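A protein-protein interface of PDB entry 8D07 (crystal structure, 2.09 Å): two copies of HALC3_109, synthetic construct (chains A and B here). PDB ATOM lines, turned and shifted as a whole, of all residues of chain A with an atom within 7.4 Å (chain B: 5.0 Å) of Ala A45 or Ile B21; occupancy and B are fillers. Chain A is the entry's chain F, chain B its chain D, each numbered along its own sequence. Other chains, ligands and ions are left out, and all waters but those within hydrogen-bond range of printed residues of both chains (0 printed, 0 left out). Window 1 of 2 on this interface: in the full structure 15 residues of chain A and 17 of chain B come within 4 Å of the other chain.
The side-chain amino group of Lys B17 is in hydrogen-bond range of the backbone carbonyl oxygen of Ala A49 (3.3 Å).
OG of Ser A41 sits at hydrogen-bond distance from O of Ala B25 (2.6 Å).
The side-chain amino group (NZ) of Lys A12 lies within salt-bridge range of the side-chain carboxylate (OE2) of Glu A15, 3.5 Å away.
Lys A12 touches Lys B17 (NZ to NZ, 3.8 Å).
OE1 of Glu A15 touches CG of Lys B17 (3.4 Å).
CD1 of Ile B21 touches CD1 of Leu A19, at 3.8 Å.
O of Ala B25 touches CD1 of Leu A38 (3.8 Å).
CA of Phe A42 touches CB of Ala B25, at 3.6 Å.
O of Ile B21 touches CB of Ala A45, 3.7 Å away.
CB of Ala A45 touches CG1 of Val B24, at 3.9 Å.
Ile B21 touches Ala A49 (CD1 to CB, 3.6 Å).
Ile B65 touches Ala A49 (CD1 to CB, 3.4 Å).
CD1 of Ile B21 touches CD2 of Leu A50, at 3.8 Å.
Of chain B, only Ile B21 and Val B24 come within 4 Å of Ala A45.
Printed residues of chain A within 4 Å of Ile B21: Leu A19 (3.8 Å), Ala A45 (3.7 Å), Ala A49 (3.6 Å) and Leu A50 (3.8 Å).
Of the printed residues of chain B, Lys A12 touches Lys B17.
Of the printed residues of chain B, Leu A19 touches Ile B21.
Of the 17 printed residues of chain A, 10 touch a printed residue of chain B.
Printed residues of chain A that touch a printed residue of chain B: Lys A12, Glu A15, Leu A19, Leu A38, Ser A41, Phe A42, Ala A45, Lys A48, Ala A49 and Leu A50.
Of the 10 printed residues of chain B, 6 touch a printed residue of chain A.
Along chain B the printed residues that touch a printed residue of chain A span positions 17 to 65.
Position printed for both chains: 19.
Of the 14 pairs that touch across the chains among the printed residues, none has its exchanged pair printed and touching as well.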
ATOM      1  N   LYS A  12     -13.719  21.357   8.940  1.00  0.00           N
ATOM      2  CA  LYS A  12     -12.917  20.666   7.938  1.00  0.00           C
ATOM      3  C   LYS A  12     -12.921  21.405   6.609  1.00  0.00           C
ATOM      4  O   LYS A  12     -11.893  21.463   5.925  1.00  0.00           O
ATOM      5  CB  LYS A  12     -13.421  19.233   7.754  1.00  0.00           C
ATOM      6  CG  LYS A  12     -12.587  18.168   8.448  1.00  0.00           C
ATOM      7  CD  LYS A  12     -11.127  18.205   8.001  1.00  0.00           C
ATOM      8  CE  LYS A  12     -10.204  17.702   9.111  1.00  0.00           C
ATOM      9  NZ  LYS A  12      -8.759  17.973   8.841  1.00  0.00           N
ATOM     10  N   GLU A  15     -10.379  24.023   6.439  1.00  0.00           N
ATOM     11  CA  GLU A  15      -9.043  23.457   6.294  1.00  0.00           C
ATOM     12  C   GLU A  15      -8.749  23.123   4.843  1.00  0.00           C
ATOM     13  O   GLU A  15      -7.767  23.604   4.260  1.00  0.00           O
ATOM     14  CB  GLU A  15      -8.923  22.192   7.142  1.00  0.00           C
ATOM     15  CG  GLU A  15      -8.541  22.417   8.569  1.00  0.00           C
ATOM     16  CD  GLU A  15      -8.543  21.125   9.346  1.00  0.00           C
ATOM     17  OE1 GLU A  15      -7.984  20.123   8.842  1.00  0.00           O
ATOM     18  OE2 GLU A  15      -9.108  21.111  10.458  1.00  0.00           O
ATOM     19  N   LEU A  16      -9.603  22.295   4.246  1.00  0.00           N
ATOM     20  CA  LEU A  16      -9.342  21.789   2.908  1.00  0.00           C
ATOM     21  C   LEU A  16      -9.291  22.914   1.883  1.00  0.00           C
ATOM     22  O   LEU A  16      -8.480  22.860   0.954  1.00  0.00           O
ATOM     23  CB  LEU A  16     -10.400  20.748   2.544  1.00  0.00           C
ATOM     24  CG  LEU A  16     -10.600  19.714   3.654  1.00  0.00           C
ATOM     25  CD1 LEU A  16     -11.664  18.702   3.276  1.00  0.00           C
ATOM     26  CD2 LEU A  16      -9.284  19.028   4.002  1.00  0.00           C
ATOM     27  N   LEU A  19      -5.910  24.697   2.381  1.00  0.00           N
ATOM     28  CA  LEU A  19      -4.884  23.813   1.835  1.00  0.00           C
ATOM     29  C   LEU A  19      -4.959  23.744   0.304  1.00  0.00           C
ATOM     30  O   LEU A  19      -3.921  23.654  -0.374  1.00  0.00           O
ATOM     31  CB  LEU A  19      -5.033  22.427   2.464  1.00  0.00           C
ATOM     32  CG  LEU A  19      -4.676  22.271   3.944  1.00  0.00           C
ATOM     33  CD1 LEU A  19      -5.084  20.903   4.453  1.00  0.00           C
ATOM     34  CD2 LEU A  19      -3.182  22.465   4.165  1.00  0.00           C
ATOM     35  N   LEU A  38       9.571  22.591  -1.933  1.00  0.00           N
ATOM     36  CA  LEU A  38       8.457  22.924  -1.041  1.00  0.00           C
ATOM     37  C   LEU A  38       7.161  22.302  -1.551  1.00  0.00           C
ATOM     38  O   LEU A  38       6.330  21.847  -0.753  1.00  0.00           O
ATOM     39  CB  LEU A  38       8.323  24.444  -0.896  1.00  0.00           C
ATOM     40  CG  LEU A  38       7.269  25.035   0.065  1.00  0.00           C
ATOM     41  CD1 LEU A  38       7.258  24.335   1.455  1.00  0.00           C
ATOM     42  CD2 LEU A  38       7.523  26.537   0.207  1.00  0.00           C
ATOM     43  N   TYR A  39       6.980  22.241  -2.877  1.00  0.00           N
ATOM     44  CA  TYR A  39       5.777  21.617  -3.436  1.00  0.00           C
ATOM     45  C   TYR A  39       5.678  20.171  -2.990  1.00  0.00           C
ATOM     46  O   TYR A  39       4.648  19.739  -2.459  1.00  0.00           O
ATOM     47  CB  TYR A  39       5.786  21.734  -4.962  1.00  0.00           C
ATOM     48  CG  TYR A  39       4.724  20.936  -5.736  1.00  0.00           C
ATOM     49  CD1 TYR A  39       3.366  21.066  -5.451  1.00  0.00           C
ATOM     50  CD2 TYR A  39       5.091  20.086  -6.775  1.00  0.00           C
ATOM     51  CE1 TYR A  39       2.411  20.365  -6.162  1.00  0.00           C
ATOM     52  CE2 TYR A  39       4.133  19.378  -7.512  1.00  0.00           C
ATOM     53  CZ  TYR A  39       2.797  19.521  -7.198  1.00  0.00           C
ATOM     54  OH  TYR A  39       1.833  18.825  -7.897  1.00  0.00           O
ATOM     55  N   GLU A  40       6.778  19.425  -3.122  1.00  0.00           N
ATOM     56  CA  GLU A  40       6.809  18.040  -2.662  1.00  0.00           C
ATOM     57  C   GLU A  40       6.708  17.925  -1.140  1.00  0.00           C
ATOM     58  O   GLU A  40       6.004  17.043  -0.631  1.00  0.00           O
ATOM     59  CB  GLU A  40       8.093  17.365  -3.158  1.00  0.00           C
ATOM     60  CG  GLU A  40       8.050  17.000  -4.655  1.00  0.00           C
ATOM     61  CD  GLU A  40       9.442  16.963  -5.302  1.00  0.00           C
ATOM     62  OE1 GLU A  40      10.452  16.834  -4.569  1.00  0.00           O
ATOM     63  OE2 GLU A  40       9.525  17.063  -6.541  1.00  0.00           O
ATOM     64  N   SER A  41       7.420  18.775  -0.393  1.00  0.00           N
ATOM     65  CA  SER A  41       7.250  18.788   1.065  1.00  0.00           C
ATOM     66  C   SER A  41       5.792  18.980   1.462  1.00  0.00           C
ATOM     67  O   SER A  41       5.292  18.320   2.391  1.00  0.00           O
ATOM     68  CB  SER A  41       8.078  19.912   1.684  1.00  0.00           C
ATOM     69  OG  SER A  41       8.189  19.690   3.065  1.00  0.00           O
ATOM     70  N   PHE A  42       5.101  19.904   0.793  1.00  0.00           N
ATOM     71  CA  PHE A  42       3.701  20.157   1.123  1.00  0.00           C
ATOM     72  C   PHE A  42       2.831  18.941   0.809  1.00  0.00           C
ATOM     73  O   PHE A  42       2.030  18.509   1.648  1.00  0.00           O
ATOM     74  CB  PHE A  42       3.222  21.395   0.372  1.00  0.00           C
ATOM     75  CG  PHE A  42       1.836  21.808   0.716  1.00  0.00           C
ATOM     76  CD1 PHE A  42       1.547  22.329   1.972  1.00  0.00           C
ATOM     77  CD2 PHE A  42       0.814  21.695  -0.214  1.00  0.00           C
ATOM     78  CE1 PHE A  42       0.259  22.716   2.290  1.00  0.00           C
ATOM     79  CE2 PHE A  42      -0.481  22.079   0.101  1.00  0.00           C
ATOM     80  CZ  PHE A  42      -0.763  22.586   1.341  1.00  0.00           C
ATOM     81  N   LEU A  43       3.002  18.345  -0.383  1.00  0.00           N
ATOM     82  CA  LEU A  43       2.251  17.133  -0.698  1.00  0.00           C
ATOM     83  C   LEU A  43       2.578  16.011   0.275  1.00  0.00           C
ATOM     84  O   LEU A  43       1.702  15.209   0.623  1.00  0.00           O
ATOM     85  CB  LEU A  43       2.549  16.663  -2.120  1.00  0.00           C
ATOM     86  CG  LEU A  43       2.068  17.521  -3.277  1.00  0.00           C
ATOM     87  CD1 LEU A  43       2.817  17.060  -4.517  1.00  0.00           C
ATOM     88  CD2 LEU A  43       0.565  17.363  -3.448  1.00  0.00           C
ATOM     89  N   ASP A  44       3.828  15.940   0.715  1.00  0.00           N
ATOM     90  CA  ASP A  44       4.220  14.975   1.739  1.00  0.00           C
ATOM     91  C   ASP A  44       3.581  15.295   3.100  1.00  0.00           C
ATOM     92  O   ASP A  44       3.158  14.387   3.826  1.00  0.00           O
ATOM     93  CB  ASP A  44       5.753  14.955   1.824  1.00  0.00           C
ATOM     94  CG  ASP A  44       6.273  13.970   2.855  1.00  0.00           C
ATOM     95  OD1 ASP A  44       5.575  12.975   3.155  1.00  0.00           O
ATOM     96  OD2 ASP A  44       7.381  14.212   3.380  1.00  0.00           O
ATOM     97  N   ALA A  45       3.512  16.574   3.477  1.00  0.00           N
ATOM     98  CA  ALA A  45       2.802  16.922   4.706  1.00  0.00           C
ATOM     99  C   ALA A  45       1.301  16.661   4.582  1.00  0.00           C
ATOM    100  O   ALA A  45       0.674  16.174   5.530  1.00  0.00           O
ATOM    101  CB  ALA A  45       3.054  18.390   5.063  1.00  0.00           C
ATOM    102  N   LEU A  46       0.712  16.971   3.420  1.00  0.00           N
ATOM    103  CA  LEU A  46      -0.710  16.726   3.209  1.00  0.00           C
ATOM    104  C   LEU A  46      -1.044  15.254   3.391  1.00  0.00           C
ATOM    105  O   LEU A  46      -1.996  14.898   4.098  1.00  0.00           O
ATOM    106  CB  LEU A  46      -1.114  17.173   1.806  1.00  0.00           C
ATOM    107  CG  LEU A  46      -1.481  18.635   1.552  1.00  0.00           C
ATOM    108  CD1 LEU A  46      -2.095  18.762   0.162  1.00  0.00           C
ATOM    109  CD2 LEU A  46      -2.431  19.140   2.615  1.00  0.00           C
ATOM    110  N   LYS A  47      -0.259  14.385   2.740  1.00  0.00           N
ATOM    111  CA  LYS A  47      -0.480  12.950   2.818  1.00  0.00           C
ATOM    112  C   LYS A  47      -0.387  12.462   4.256  1.00  0.00           C
ATOM    113  O   LYS A  47      -1.204  11.647   4.699  1.00  0.00           O
ATOM    114  CB  LYS A  47       0.533  12.223   1.924  1.00  0.00           C
ATOM    115  CG  LYS A  47       0.946  10.843   2.432  1.00  0.00           C
ATOM    116  CD  LYS A  47       2.445  10.594   2.293  1.00  0.00           C
ATOM    117  CE  LYS A  47       2.919   9.571   3.330  1.00  0.00           C
ATOM    118  NZ  LYS A  47       4.383   9.324   3.304  1.00  0.00           N
ATOM    119  N   LYS A  48       0.595  12.956   5.007  1.00  0.00           N
ATOM    120  CA  LYS A  48       0.738  12.526   6.396  1.00  0.00           C
ATOM    121  C   LYS A  48      -0.455  12.964   7.242  1.00  0.00           C
ATOM    122  O   LYS A  48      -0.995  12.174   8.028  1.00  0.00           O
ATOM    123  CB  LYS A  48       2.025  13.091   6.987  1.00  0.00           C
ATOM    124  CG  LYS A  48       3.284  12.368   6.557  1.00  0.00           C
ATOM    125  CD  LYS A  48       4.509  12.990   7.199  1.00  0.00           C
ATOM    126  CE  LYS A  48       5.335  11.953   7.946  1.00  0.00           C
ATOM    127  NZ  LYS A  48       6.773  12.353   8.055  1.00  0.00           N
ATOM    128  N   ALA A  49      -0.889  14.213   7.083  1.00  0.00           N
ATOM    129  CA  ALA A  49      -1.789  14.824   8.049  1.00  0.00           C
ATOM    130  C   ALA A  49      -3.259  14.511   7.799  1.00  0.00           C
ATOM    131  O   ALA A  49      -4.061  14.584   8.734  1.00  0.00           O
ATOM    132  CB  ALA A  49      -1.590  16.343   8.050  1.00  0.00           C
ATOM    133  N   LEU A  50      -3.631  14.182   6.572  1.00  0.00           N
ATOM    134  CA  LEU A  50      -5.023  14.023   6.192  1.00  0.00           C
ATOM    135  C   LEU A  50      -5.280  12.620   5.652  1.00  0.00           C
ATOM    136  O   LEU A  50      -4.389  11.982   5.078  1.00  0.00           O
ATOM    137  CB  LEU A  50      -5.418  15.055   5.137  1.00  0.00           C
ATOM    138  CG  LEU A  50      -4.832  16.465   5.187  1.00  0.00           C
ATOM    139  CD1 LEU A  50      -5.136  17.170   3.884  1.00  0.00           C
ATOM    140  CD2 LEU A  50      -5.427  17.243   6.340  1.00  0.00           C
ATOM    141  N   LYS B  17      -4.411  23.418  12.715  1.00  0.00           N
ATOM    142  CA  LYS B  17      -4.066  22.229  11.943  1.00  0.00           C
ATOM    143  C   LYS B  17      -3.533  22.591  10.560  1.00  0.00           C
ATOM    144  O   LYS B  17      -2.572  21.979  10.079  1.00  0.00           O
ATOM    145  CB  LYS B  17      -5.290  21.321  11.847  1.00  0.00           C
ATOM    146  CG  LYS B  17      -5.170  20.208  10.826  1.00  0.00           C
ATOM    147  CD  LYS B  17      -5.553  18.854  11.409  1.00  0.00           C
ATOM    148  CE  LYS B  17      -5.101  17.732  10.486  1.00  0.00           C
ATOM    149  NZ  LYS B  17      -5.850  16.468  10.729  1.00  0.00           N
ATOM    150  N   VAL B  18      -4.138  23.577   9.895  1.00  0.00           N
ATOM    151  CA  VAL B  18      -3.600  24.012   8.609  1.00  0.00           C
ATOM    152  C   VAL B  18      -2.202  24.576   8.786  1.00  0.00           C
ATOM    153  O   VAL B  18      -1.294  24.277   8.001  1.00  0.00           O
ATOM    154  CB  VAL B  18      -4.516  25.053   7.946  1.00  0.00           C
ATOM    155  CG1 VAL B  18      -3.760  25.718   6.781  1.00  0.00           C
ATOM    156  CG2 VAL B  18      -5.795  24.410   7.481  1.00  0.00           C
ATOM    157  N   LEU B  19      -2.014  25.405   9.814  1.00  0.00           N
ATOM    158  CA  LEU B  19      -0.725  26.059  10.023  1.00  0.00           C
ATOM    159  C   LEU B  19       0.353  25.051  10.397  1.00  0.00           C
ATOM    160  O   LEU B  19       1.531  25.253  10.073  1.00  0.00           O
ATOM    161  CB  LEU B  19      -0.853  27.135  11.109  1.00  0.00           C
ATOM    162  CG  LEU B  19      -1.715  28.328  10.673  1.00  0.00           C
ATOM    163  CD1 LEU B  19      -2.025  29.263  11.855  1.00  0.00           C
ATOM    164  CD2 LEU B  19      -0.989  29.082   9.573  1.00  0.00           C
ATOM    165  N   ALA B  20      -0.026  23.968  11.092  1.00  0.00           N
ATOM    166  CA  ALA B  20       0.940  22.915  11.402  1.00  0.00           C
ATOM    167  C   ALA B  20       1.341  22.152  10.143  1.00  0.00           C
ATOM    168  O   ALA B  20       2.486  21.698  10.011  1.00  0.00           O
ATOM    169  CB  ALA B  20       0.360  21.962  12.446  1.00  0.00           C
ATOM    170  N   ILE B  21       0.412  21.996   9.205  1.00  0.00           N
ATOM    171  CA  ILE B  21       0.753  21.342   7.950  1.00  0.00           C
ATOM    172  C   ILE B  21       1.738  22.203   7.176  1.00  0.00           C
ATOM    173  O   ILE B  21       2.750  21.706   6.660  1.00  0.00           O
ATOM    174  CB  ILE B  21      -0.524  21.048   7.148  1.00  0.00           C
ATOM    175  CG1 ILE B  21      -1.369  20.022   7.895  1.00  0.00           C
ATOM    176  CG2 ILE B  21      -0.176  20.551   5.732  1.00  0.00           C
ATOM    177  CD1 ILE B  21      -2.669  19.705   7.200  1.00  0.00           C
ATOM    178  N   VAL B  22       1.483  23.519   7.121  1.00  0.00           N
ATOM    179  CA  VAL B  22       2.427  24.420   6.458  1.00  0.00           C
ATOM    180  C   VAL B  22       3.768  24.394   7.173  1.00  0.00           C
ATOM    181  O   VAL B  22       4.832  24.391   6.539  1.00  0.00           O
ATOM    182  CB  VAL B  22       1.863  25.847   6.392  1.00  0.00           C
ATOM    183  CG1 VAL B  22       2.882  26.785   5.754  1.00  0.00           C
ATOM    184  CG2 VAL B  22       0.557  25.882   5.640  1.00  0.00           C
ATOM    185  N   LEU B  23       3.748  24.370   8.502  1.00  0.00           N
ATOM    186  CA  LEU B  23       5.011  24.353   9.237  1.00  0.00           C
ATOM    187  C   LEU B  23       5.825  23.104   8.916  1.00  0.00           C
ATOM    188  O   LEU B  23       7.029  23.193   8.657  1.00  0.00           O
ATOM    189  CB  LEU B  23       4.757  24.450  10.744  1.00  0.00           C
ATOM    190  CG  LEU B  23       6.021  24.413  11.619  1.00  0.00           C
ATOM    191  CD1 LEU B  23       7.021  25.482  11.167  1.00  0.00           C
ATOM    192  CD2 LEU B  23       5.651  24.612  13.094  1.00  0.00           C
ATOM    193  N   VAL B  24       5.193  21.927   8.954  1.00  0.00           N
ATOM    194  CA  VAL B  24       5.887  20.684   8.589  1.00  0.00           C
ATOM    195  C   VAL B  24       6.566  20.811   7.229  1.00  0.00           C
ATOM    196  O   VAL B  24       7.736  20.440   7.060  1.00  0.00           O
ATOM    197  CB  VAL B  24       4.911  19.496   8.593  1.00  0.00           C
ATOM    198  CG1 VAL B  24       5.588  18.270   7.986  1.00  0.00           C
ATOM    199  CG2 VAL B  24       4.435  19.198  10.020  1.00  0.00           C
ATOM    200  N   ALA B  25       5.840  21.340   6.232  1.00  0.00           N
ATOM    201  CA  ALA B  25       6.376  21.402   4.873  1.00  0.00           C
ATOM    202  C   ALA B  25       7.564  22.352   4.793  1.00  0.00           C
ATOM    203  O   ALA B  25       8.594  22.023   4.196  1.00  0.00           O
ATOM    204  CB  ALA B  25       5.282  21.821   3.886  1.00  0.00           C
ATOM    205  N   ILE B  65       2.646  15.199  13.132  1.00  0.00           N
ATOM    206  CA  ILE B  65       2.687  14.912  11.701  1.00  0.00           C
ATOM    207  C   ILE B  65       4.061  14.396  11.293  1.00  0.00           C
ATOM    208  O   ILE B  65       4.175  13.470  10.482  1.00  0.00           O
ATOM    209  CB  ILE B  65       2.297  16.171  10.906  1.00  0.00           C
ATOM    210  CG1 ILE B  65       0.915  16.649  11.351  1.00  0.00           C
ATOM    211  CG2 ILE B  65       2.303  15.882   9.413  1.00  0.00           C
ATOM    212  CD1 ILE B  65       0.323  17.737  10.505  1.00  0.00           C
